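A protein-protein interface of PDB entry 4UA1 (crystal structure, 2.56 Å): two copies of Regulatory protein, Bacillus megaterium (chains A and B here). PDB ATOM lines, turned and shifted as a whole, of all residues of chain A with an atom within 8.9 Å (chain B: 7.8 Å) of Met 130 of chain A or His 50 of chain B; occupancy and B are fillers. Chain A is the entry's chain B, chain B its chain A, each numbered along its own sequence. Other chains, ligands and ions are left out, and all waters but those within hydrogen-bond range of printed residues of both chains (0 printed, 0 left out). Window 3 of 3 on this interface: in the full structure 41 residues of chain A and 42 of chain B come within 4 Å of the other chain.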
ATOM      1  N   LEU A 110      26.943  36.722  -9.444  1.00  0.00           N
ATOM      2  CA  LEU A 110      27.482  36.119 -10.650  1.00  0.00           C
ATOM      3  C   LEU A 110      27.814  37.145 -11.753  1.00  0.00           C
ATOM      4  O   LEU A 110      28.944  37.197 -12.243  1.00  0.00           O
ATOM      5  CB  LEU A 110      26.486  35.111 -11.177  1.00  0.00           C
ATOM      6  CG  LEU A 110      26.563  33.812 -10.408  1.00  0.00           C
ATOM      7  CD1 LEU A 110      25.348  32.917 -10.716  1.00  0.00           C
ATOM      8  CD2 LEU A 110      27.883  33.159 -10.794  1.00  0.00           C
ATOM      9  N   TYR A 121      36.249  34.785 -24.537  1.00  0.00           N
ATOM     10  CA  TYR A 121      35.689  33.433 -24.402  1.00  0.00           C
ATOM     11  C   TYR A 121      35.425  33.093 -22.932  1.00  0.00           C
ATOM     12  O   TYR A 121      34.485  32.361 -22.611  1.00  0.00           O
ATOM     13  CB  TYR A 121      36.613  32.381 -24.996  1.00  0.00           C
ATOM     14  CG  TYR A 121      36.628  32.349 -26.489  1.00  0.00           C
ATOM     15  CD1 TYR A 121      37.519  31.522 -27.174  1.00  0.00           C
ATOM     16  CD2 TYR A 121      35.753  33.136 -27.230  1.00  0.00           C
ATOM     17  CE1 TYR A 121      37.537  31.478 -28.551  1.00  0.00           C
ATOM     18  CE2 TYR A 121      35.767  33.105 -28.613  1.00  0.00           C
ATOM     19  CZ  TYR A 121      36.660  32.271 -29.267  1.00  0.00           C
ATOM     20  OH  TYR A 121      36.680  32.230 -30.643  1.00  0.00           O
ATOM     21  N   CYS A 123      34.060  33.541 -19.485  1.00  0.00           N
ATOM     22  CA  CYS A 123      33.065  34.235 -18.705  1.00  0.00           C
ATOM     23  C   CYS A 123      33.063  33.693 -17.285  1.00  0.00           C
ATOM     24  O   CYS A 123      32.845  32.499 -17.080  1.00  0.00           O
ATOM     25  CB  CYS A 123      31.691  34.082 -19.340  1.00  0.00           C
ATOM     26  SG  CYS A 123      30.431  34.656 -18.260  1.00  0.00           S
ATOM     27  N   PRO A 124      33.353  34.562 -16.304  1.00  0.00           N
ATOM     28  CA  PRO A 124      33.364  34.163 -14.881  1.00  0.00           C
ATOM     29  C   PRO A 124      32.033  33.533 -14.442  1.00  0.00           C
ATOM     30  O   PRO A 124      32.018  32.710 -13.528  1.00  0.00           O
ATOM     31  CB  PRO A 124      33.634  35.480 -14.135  1.00  0.00           C
ATOM     32  CG  PRO A 124      34.307  36.368 -15.151  1.00  0.00           C
ATOM     33  CD  PRO A 124      33.700  35.981 -16.495  1.00  0.00           C
ATOM     34  N   ILE A 125      30.935  33.926 -15.092  1.00  0.00           N
ATOM     35  CA  ILE A 125      29.651  33.340 -14.786  1.00  0.00           C
ATOM     36  C   ILE A 125      29.727  31.857 -15.128  1.00  0.00           C
ATOM     37  O   ILE A 125      29.464  30.992 -14.288  1.00  0.00           O
ATOM     38  CB  ILE A 125      28.496  33.989 -15.572  1.00  0.00           C
ATOM     39  CG1 ILE A 125      28.379  35.493 -15.282  1.00  0.00           C
ATOM     40  CG2 ILE A 125      27.163  33.296 -15.240  1.00  0.00           C
ATOM     41  CD1 ILE A 125      27.171  36.174 -15.989  1.00  0.00           C
ATOM     42  N   ILE A 126      30.099  31.569 -16.372  1.00  0.00           N
ATOM     43  CA  ILE A 126      30.147  30.198 -16.848  1.00  0.00           C
ATOM     44  C   ILE A 126      31.174  29.391 -16.071  1.00  0.00           C
ATOM     45  O   ILE A 126      30.917  28.263 -15.649  1.00  0.00           O
ATOM     46  CB  ILE A 126      30.461  30.136 -18.350  1.00  0.00           C
ATOM     47  CG1 ILE A 126      29.350  30.832 -19.146  1.00  0.00           C
ATOM     48  CG2 ILE A 126      30.603  28.682 -18.801  1.00  0.00           C
ATOM     49  CD1 ILE A 126      29.657  30.997 -20.625  1.00  0.00           C
ATOM     50  N   GLU A 127      32.339  29.985 -15.876  1.00  0.00           N
ATOM     51  CA  GLU A 127      33.370  29.317 -15.127  1.00  0.00           C
ATOM     52  C   GLU A 127      32.880  28.985 -13.734  1.00  0.00           C
ATOM     53  O   GLU A 127      33.070  27.853 -13.283  1.00  0.00           O
ATOM     54  CB  GLU A 127      34.620  30.177 -15.064  1.00  0.00           C
ATOM     55  CG  GLU A 127      35.253  30.383 -16.426  1.00  0.00           C
ATOM     56  CD  GLU A 127      36.367  31.400 -16.397  1.00  0.00           C
ATOM     57  OE1 GLU A 127      37.185  31.389 -17.336  1.00  0.00           O
ATOM     58  OE2 GLU A 127      36.409  32.231 -15.458  1.00  0.00           O
ATOM     59  N   THR A 128      32.183  29.927 -13.091  1.00  0.00           N
ATOM     60  CA  THR A 128      31.729  29.704 -11.721  1.00  0.00           C
ATOM     61  C   THR A 128      30.716  28.589 -11.648  1.00  0.00           C
ATOM     62  O   THR A 128      30.866  27.658 -10.848  1.00  0.00           O
ATOM     63  CB  THR A 128      31.092  30.963 -11.077  1.00  0.00           C
ATOM     64  OG1 THR A 128      32.097  31.972 -10.917  1.00  0.00           O
ATOM     65  CG2 THR A 128      30.541  30.626  -9.709  1.00  0.00           C
ATOM     66  N   LEU A 129      29.717  28.658 -12.519  1.00  0.00           N
ATOM     67  CA  LEU A 129      28.665  27.646 -12.557  1.00  0.00           C
ATOM     68  C   LEU A 129      29.162  26.274 -13.052  1.00  0.00           C
ATOM     69  O   LEU A 129      28.478  25.272 -12.896  1.00  0.00           O
ATOM     70  CB  LEU A 129      27.539  28.137 -13.440  1.00  0.00           C
ATOM     71  CG  LEU A 129      26.841  29.350 -12.837  1.00  0.00           C
ATOM     72  CD1 LEU A 129      25.643  29.719 -13.705  1.00  0.00           C
ATOM     73  CD2 LEU A 129      26.436  29.085 -11.389  1.00  0.00           C
ATOM     74  N   MET A 130      30.339  26.253 -13.676  1.00  0.00           N
ATOM     75  CA  MET A 130      30.921  25.022 -14.181  1.00  0.00           C
ATOM     76  C   MET A 130      31.587  24.227 -13.074  1.00  0.00           C
ATOM     77  O   MET A 130      31.594  23.000 -13.115  1.00  0.00           O
ATOM     78  CB  MET A 130      31.942  25.304 -15.294  1.00  0.00           C
ATOM     79  CG  MET A 130      31.297  25.392 -16.647  1.00  0.00           C
ATOM     80  SD  MET A 130      32.421  25.495 -18.025  1.00  0.00           S
ATOM     81  CE  MET A 130      31.306  24.903 -19.312  1.00  0.00           C
ATOM     82  N   LYS A 131      32.155  24.942 -12.100  1.00  0.00           N
ATOM     83  CA  LYS A 131      32.885  24.329 -10.992  1.00  0.00           C
ATOM     84  C   LYS A 131      31.906  23.727  -9.980  1.00  0.00           C
ATOM     85  O   LYS A 131      32.268  23.406  -8.847  1.00  0.00           O
ATOM     86  CB  LYS A 131      33.804  25.357 -10.315  1.00  0.00           C
ATOM     87  N   ALA B   9      28.667  10.025 -14.732  1.00  0.00           N
ATOM     88  CA  ALA B   9      28.346  11.408 -15.103  1.00  0.00           C
ATOM     89  C   ALA B   9      27.095  11.871 -14.377  1.00  0.00           C
ATOM     90  O   ALA B   9      26.832  13.064 -14.273  1.00  0.00           O
ATOM     91  CB  ALA B   9      28.161  11.555 -16.602  1.00  0.00           C
ATOM     92  N   LYS B  11      27.066  11.859 -11.417  1.00  0.00           N
ATOM     93  CA  LYS B  11      27.731  12.592 -10.319  1.00  0.00           C
ATOM     94  C   LYS B  11      27.496  14.102 -10.424  1.00  0.00           C
ATOM     95  O   LYS B  11      28.037  14.874  -9.648  1.00  0.00           O
ATOM     96  CB  LYS B  11      29.230  12.380 -10.336  1.00  0.00           C
ATOM     97  N   CYS B  12      26.751  14.535 -11.434  1.00  0.00           N
ATOM     98  CA  CYS B  12      26.359  15.933 -11.555  1.00  0.00           C
ATOM     99  C   CYS B  12      25.034  16.171 -10.852  1.00  0.00           C
ATOM    100  O   CYS B  12      24.480  17.268 -10.896  1.00  0.00           O
ATOM    101  CB  CYS B  12      26.231  16.324 -13.026  1.00  0.00           C
ATOM    102  SG  CYS B  12      27.766  16.547 -13.909  1.00  0.00           S
ATOM    103  N   GLY B  13      24.510  15.125 -10.225  1.00  0.00           N
ATOM    104  CA  GLY B  13      23.241  15.220  -9.537  1.00  0.00           C
ATOM    105  C   GLY B  13      22.068  15.174 -10.481  1.00  0.00           C
ATOM    106  O   GLY B  13      21.018  15.724 -10.190  1.00  0.00           O
ATOM    107  N   VAL B  14      22.241  14.522 -11.622  1.00  0.00           N
ATOM    108  CA  VAL B  14      21.141  14.337 -12.567  1.00  0.00           C
ATOM    109  C   VAL B  14      20.989  12.858 -12.923  1.00  0.00           C
ATOM    110  O   VAL B  14      21.974  12.200 -13.270  1.00  0.00           O
ATOM    111  CB  VAL B  14      21.333  15.163 -13.859  1.00  0.00           C
ATOM    112  CG1 VAL B  14      20.087  15.078 -14.723  1.00  0.00           C
ATOM    113  CG2 VAL B  14      21.659  16.611 -13.522  1.00  0.00           C
ATOM    114  N   GLN B  43      34.448  14.807 -20.526  1.00  0.00           N
ATOM    115  CA  GLN B  43      34.798  15.692 -19.423  1.00  0.00           C
ATOM    116  C   GLN B  43      34.287  17.101 -19.608  1.00  0.00           C
ATOM    117  O   GLN B  43      33.907  17.769 -18.640  1.00  0.00           O
ATOM    118  CB  GLN B  43      36.310  15.744 -19.255  1.00  0.00           C
ATOM    119  CG  GLN B  43      36.822  16.691 -18.166  1.00  0.00           C
ATOM    120  CD  GLN B  43      36.407  16.294 -16.778  1.00  0.00           C
ATOM    121  OE1 GLN B  43      36.583  15.149 -16.395  1.00  0.00           O
ATOM    122  NE2 GLN B  43      35.945  17.247 -15.985  1.00  0.00           N
ATOM    123  N   GLN B  44      34.282  17.562 -20.848  1.00  0.00           N
ATOM    124  CA  GLN B  44      33.819  18.901 -21.128  1.00  0.00           C
ATOM    125  C   GLN B  44      32.309  18.810 -21.045  1.00  0.00           C
ATOM    126  O   GLN B  44      31.586  19.819 -20.878  1.00  0.00           O
ATOM    127  CB  GLN B  44      34.292  19.378 -22.503  1.00  0.00           C
ATOM    128  CG  GLN B  44      35.736  18.998 -22.838  1.00  0.00           C
ATOM    129  N   THR B  45      31.840  17.570 -21.127  1.00  0.00           N
ATOM    130  CA  THR B  45      30.424  17.285 -20.974  1.00  0.00           C
ATOM    131  C   THR B  45      30.069  17.400 -19.502  1.00  0.00           C
ATOM    132  O   THR B  45      28.966  17.838 -19.154  1.00  0.00           O
ATOM    133  CB  THR B  45      30.053  15.875 -21.533  1.00  0.00           C
ATOM    134  OG1 THR B  45      30.329  15.830 -22.936  1.00  0.00           O
ATOM    135  CG2 THR B  45      28.588  15.578 -21.355  1.00  0.00           C
ATOM    136  N   VAL B  46      31.015  17.041 -18.638  1.00  0.00           N
ATOM    137  CA  VAL B  46      30.806  17.157 -17.201  1.00  0.00           C
ATOM    138  C   VAL B  46      30.581  18.616 -16.839  1.00  0.00           C
ATOM    139  O   VAL B  46      29.581  18.971 -16.170  1.00  0.00           O
ATOM    140  CB  VAL B  46      31.994  16.591 -16.406  1.00  0.00           C
ATOM    141  CG1 VAL B  46      31.848  16.888 -14.909  1.00  0.00           C
ATOM    142  CG2 VAL B  46      32.104  15.105 -16.644  1.00  0.00           C
ATOM    143  N   ASP B  47      31.482  19.466 -17.336  1.00  0.00           N
ATOM    144  CA  ASP B  47      31.361  20.903 -17.144  1.00  0.00           C
ATOM    145  C   ASP B  47      30.013  21.400 -17.703  1.00  0.00           C
ATOM    146  O   ASP B  47      29.272  22.089 -17.011  1.00  0.00           O
ATOM    147  CB  ASP B  47      32.508  21.661 -17.829  1.00  0.00           C
ATOM    148  CG  ASP B  47      33.889  21.353 -17.237  1.00  0.00           C
ATOM    149  OD1 ASP B  47      34.878  21.640 -17.929  1.00  0.00           O
ATOM    150  OD2 ASP B  47      34.011  20.857 -16.099  1.00  0.00           O
ATOM    151  N   ARG B  48      29.670  21.011 -18.927  1.00  0.00           N
ATOM    152  CA  ARG B  48      28.467  21.551 -19.521  1.00  0.00           C
ATOM    153  C   ARG B  48      27.205  21.157 -18.759  1.00  0.00           C
ATOM    154  O   ARG B  48      26.307  21.977 -18.547  1.00  0.00           O
ATOM    155  CB  ARG B  48      28.374  21.110 -20.973  1.00  0.00           C
ATOM    156  CG  ARG B  48      27.243  21.744 -21.764  1.00  0.00           C
ATOM    157  CD  ARG B  48      27.486  21.442 -23.218  1.00  0.00           C
ATOM    158  NE  ARG B  48      26.458  21.967 -24.107  1.00  0.00           N
ATOM    159  CZ  ARG B  48      26.590  23.068 -24.840  1.00  0.00           C
ATOM    160  NH1 ARG B  48      27.697  23.799 -24.781  1.00  0.00           N
ATOM    161  NH2 ARG B  48      25.598  23.441 -25.630  1.00  0.00           N
ATOM    162  N   LEU B  49      27.159  19.911 -18.304  1.00  0.00           N
ATOM    163  CA  LEU B  49      26.011  19.428 -17.549  1.00  0.00           C
ATOM    164  C   LEU B  49      25.910  20.101 -16.169  1.00  0.00           C
ATOM    165  O   LEU B  49      24.798  20.404 -15.718  1.00  0.00           O
ATOM    166  CB  LEU B  49      26.081  17.908 -17.423  1.00  0.00           C
ATOM    167  CG  LEU B  49      24.847  17.221 -16.850  1.00  0.00           C
ATOM    168  CD1 LEU B  49      23.617  17.653 -17.587  1.00  0.00           C
ATOM    169  CD2 LEU B  49      25.026  15.728 -16.981  1.00  0.00           C
ATOM    170  N   HIS B  50      27.051  20.373 -15.528  1.00  0.00           N
ATOM    171  CA  HIS B  50      27.038  21.199 -14.316  1.00  0.00           C
ATOM    172  C   HIS B  50      26.383  22.526 -14.635  1.00  0.00           C
ATOM    173  O   HIS B  50      25.507  23.004 -13.913  1.00  0.00           O
ATOM    174  CB  HIS B  50      28.447  21.504 -13.783  1.00  0.00           C
ATOM    175  CG  HIS B  50      29.033  20.432 -12.927  1.00  0.00           C
ATOM    176  ND1 HIS B  50      28.411  19.954 -11.795  1.00  0.00           N
ATOM    177  CD2 HIS B  50      30.212  19.772 -13.020  1.00  0.00           C
ATOM    178  CE1 HIS B  50      29.163  19.015 -11.249  1.00  0.00           C
ATOM    179  NE2 HIS B  50      30.265  18.893 -11.969  1.00  0.00           N
ATOM    180  N   PHE B  51      26.854  23.124 -15.718  1.00  0.00           N
ATOM    181  CA  PHE B  51      26.401  24.434 -16.144  1.00  0.00           C
ATOM    182  C   PHE B  51      24.883  24.417 -16.295  1.00  0.00           C
ATOM    183  O   PHE B  51      24.192  25.321 -15.805  1.00  0.00           O
ATOM    184  CB  PHE B  51      27.125  24.837 -17.443  1.00  0.00           C
ATOM    185  CG  PHE B  51      26.769  26.208 -17.966  1.00  0.00           C
ATOM    186  CD1 PHE B  51      26.491  27.257 -17.103  1.00  0.00           C
ATOM    187  CD2 PHE B  51      26.737  26.447 -19.337  1.00  0.00           C
ATOM    188  CE1 PHE B  51      26.162  28.514 -17.599  1.00  0.00           C
ATOM    189  CE2 PHE B  51      26.420  27.706 -19.837  1.00  0.00           C
ATOM    190  CZ  PHE B  51      26.127  28.733 -18.970  1.00  0.00           C
ATOM    191  N   ILE B  52      24.370  23.367 -16.937  1.00  0.00           N
ATOM    192  CA  ILE B  52      22.945  23.303 -17.261  1.00  0.00           C
ATOM    193  C   ILE B  52      22.148  23.171 -15.961  1.00  0.00           C
ATOM    194  O   ILE B  52      21.188  23.912 -15.715  1.00  0.00           O
ATOM    195  CB  ILE B  52      22.628  22.127 -18.257  1.00  0.00           C
ATOM    196  CG1 ILE B  52      23.228  22.417 -19.633  1.00  0.00           C
ATOM    197  CG2 ILE B  52      21.121  21.888 -18.381  1.00  0.00           C
ATOM    198  CD1 ILE B  52      23.282  21.213 -20.551  1.00  0.00           C
ATOM    199  N   LYS B  53      22.590  22.243 -15.118  1.00  0.00           N
ATOM    200  CA  LYS B  53      21.982  22.005 -13.823  1.00  0.00           C
ATOM    201  C   LYS B  53      21.885  23.274 -12.987  1.00  0.00           C
ATOM    202  O   LYS B  53      20.817  23.599 -12.448  1.00  0.00           O
ATOM    203  CB  LYS B  53      22.800  20.958 -13.067  1.00  0.00           C
ATOM    204  CG  LYS B  53      22.324  20.620 -11.656  1.00  0.00           C
ATOM    205  CD  LYS B  53      20.968  19.926 -11.665  1.00  0.00           C
ATOM    206  CE  LYS B  53      20.591  19.555 -10.249  1.00  0.00           C
ATOM    207  NZ  LYS B  53      21.823  19.135  -9.513  1.00  0.00           N
ATOM    208  N   ARG B  54      22.992  24.000 -12.870  1.00  0.00           N
ATOM    209  CA  ARG B  54      22.970  25.156 -11.993  1.00  0.00           C
ATOM    210  C   ARG B  54      22.148  26.254 -12.611  1.00  0.00           C
ATOM    211  O   ARG B  54      21.440  26.967 -11.892  1.00  0.00           O
ATOM    212  CB  ARG B  54      24.379  25.610 -11.620  1.00  0.00           C
ATOM    213  CG  ARG B  54      24.984  24.651 -10.617  1.00  0.00           C
ATOM    214  CD  ARG B  54      26.479  24.682 -10.596  1.00  0.00           C
ATOM    215  NE  ARG B  54      27.065  23.476  -9.992  1.00  0.00           N
ATOM    216  CZ  ARG B  54      28.324  23.111 -10.188  1.00  0.00           C
ATOM    217  NH1 ARG B  54      29.083  23.863 -10.954  1.00  0.00           N
ATOM    218  NH2 ARG B  54      28.823  22.025  -9.612  1.00  0.00           N
ATOM    219  N   MET B  55      22.143  26.352 -13.935  1.00  0.00           N
ATOM    220  CA  MET B  55      21.259  27.346 -14.552  1.00  0.00           C
ATOM    221  C   MET B  55      19.796  27.039 -14.192  1.00  0.00           C
ATOM    222  O   MET B  55      19.003  27.934 -13.900  1.00  0.00           O
ATOM    223  CB  MET B  55      21.469  27.400 -16.069  1.00  0.00           C
ATOM    224  CG  MET B  55      22.705  28.232 -16.472  1.00  0.00           C
ATOM    225  SD  MET B  55      22.626  28.786 -18.183  1.00  0.00           S
ATOM    226  CE  MET B  55      22.681  27.205 -19.042  1.00  0.00           C
ATOM    227  N   GLN B  56      19.441  25.762 -14.184  1.00  0.00           N
ATOM    228  CA  GLN B  56      18.089  25.404 -13.795  1.00  0.00           C
ATOM    229  C   GLN B  56      17.825  25.673 -12.313  1.00  0.00           C
ATOM    230  O   GLN B  56      16.700  26.014 -11.923  1.00  0.00           O
ATOM    231  CB  GLN B  56      17.809  23.953 -14.132  1.00  0.00           C
ATOM    232  CG  GLN B  56      17.292  23.801 -15.526  1.00  0.00           C
ATOM    233  CD  GLN B  56      17.163  22.368 -15.932  1.00  0.00           C
ATOM    234  OE1 GLN B  56      18.158  21.677 -16.138  1.00  0.00           O
ATOM    235  NE2 GLN B  56      15.931  21.891 -16.008  1.00  0.00           N
ATOM    236  N   GLU B  57      18.858  25.547 -11.484  1.00  0.00           N
ATOM    237  CA  GLU B  57      18.686  25.863 -10.074  1.00  0.00           C
ATOM    238  C   GLU B  57      18.546  27.374  -9.901  1.00  0.00           C
ATOM    239  O   GLU B  57      18.046  27.845  -8.888  1.00  0.00           O
ATOM    240  CB  GLU B  57      19.852  25.313  -9.260  1.00  0.00           C
ATOM    241  CG  GLU B  57      19.960  23.800  -9.347  1.00  0.00           C
ATOM    242  CD  GLU B  57      21.206  23.250  -8.680  1.00  0.00           C
ATOM    243  OE1 GLU B  57      22.205  23.998  -8.565  1.00  0.00           O
ATOM    244  OE2 GLU B  57      21.180  22.063  -8.281  1.00  0.00           O
ATOM    245  N   LEU B  69      22.440  28.344 -25.037  1.00  0.00           N
ATOM    246  CA  LEU B  69      23.576  27.523 -25.427  1.00  0.00           C
ATOM    247  C   LEU B  69      23.824  27.673 -26.912  1.00  0.00           C
ATOM    248  O   LEU B  69      24.970  27.629 -27.344  1.00  0.00           O
ATOM    249  CB  LEU B  69      23.358  26.045 -25.098  1.00  0.00           C
ATOM    250  CG  LEU B  69      23.545  25.535 -23.666  1.00  0.00           C
ATOM    251  CD1 LEU B  69      23.227  24.043 -23.591  1.00  0.00           C
ATOM    252  CD2 LEU B  69      24.941  25.832 -23.122  1.00  0.00           C
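No position is printed for both chains.
Among the printed residues, merely in contact across the chains: Met 130 of chain A with His 50 of chain B, Met 130 of chain A with Asp 47 of chain B, Ile 126 of chain A with Phe 51 of chain B, Leu 129 of chain A with His 50 of chain B and Leu 129 of chain A with Phe 51 of chain B.
N of Ile 126 of chain A sits close to SG of Cys 123 of chain A (3.6 Å).
ND1 of His 50 of chain B sits at hydrogen-bond distance from NH2 of Arg 54 of chain B, 3.0 Å away.
Of the printed residues of chain B, Met 130 of chain A touches Asp 47 (3.8 Å), His 50 (3.5 Å) and Arg 54 (3.3 Å).
Of the printed residues of chain B, Lys 131 of chain A touches Arg 54 (3.0 Å).
Of chain A, only Met 130 comes within 4 Å of Asp 47 of chain B.
His 50 of chain B touches two residues of chain A.
Of the printed residues of chain A, Phe 51 of chain B touches Ile 126 and Leu 129.
Of the printed residues of chain A, Arg 54 of chain B touches Leu 129 (2.5 Å), Met 130 (3.3 Å) and Lys 131 (3.0 Å).
The nearest residue of chain B that does not touch Met 130 of chain A is Arg 48 of chain B (4.2 Å).
The nearest residue of chain A that does not touch His 50 of chain B is Lys 131 of chain A (5.3 Å).
Of the 21 printed residues of chain B, 4 touch a printed residue of chain A.
Printed residues of chain B that touch a printed residue of chain A: Asp 47, His 50, Phe 51 and Arg 54.
Hydrophobic or aromatic side chains of chain B within 4 Å of the printed part of chain A: His 50 and Phe 51.
Of the 11 printed residues of chain A, 4 touch a printed residue of chain B.
Hydrophobic or aromatic side chains of chain A that line the printed part of chain B: Ile 126, Leu 129 and Met 130.
Along chain A the printed residues that touch a printed residue of chain B span positions 126 to 131.
Among the printed residues, 8 pairs touch across the chains.
Among the printed residues, no Asp or Glu carboxylate lies within 4 Å of a Lys or Arg side-chain nitrogen of the other chain.
The guanidinium group (NH1) of Arg 54 of chain B sits close to the backbone carbonyl oxygen (O) of Met 130 of chain A, 3.4 Å away.
The backbone carbonyl oxygen of Leu 129 of chain A lies within hydrogen-bond range of the guanidinium group of Arg 54 of chain B, at 2.5 Å.
The backbone NH of Lys 131 of chain A sits close to the guanidinium group of Arg 54 of chain B.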
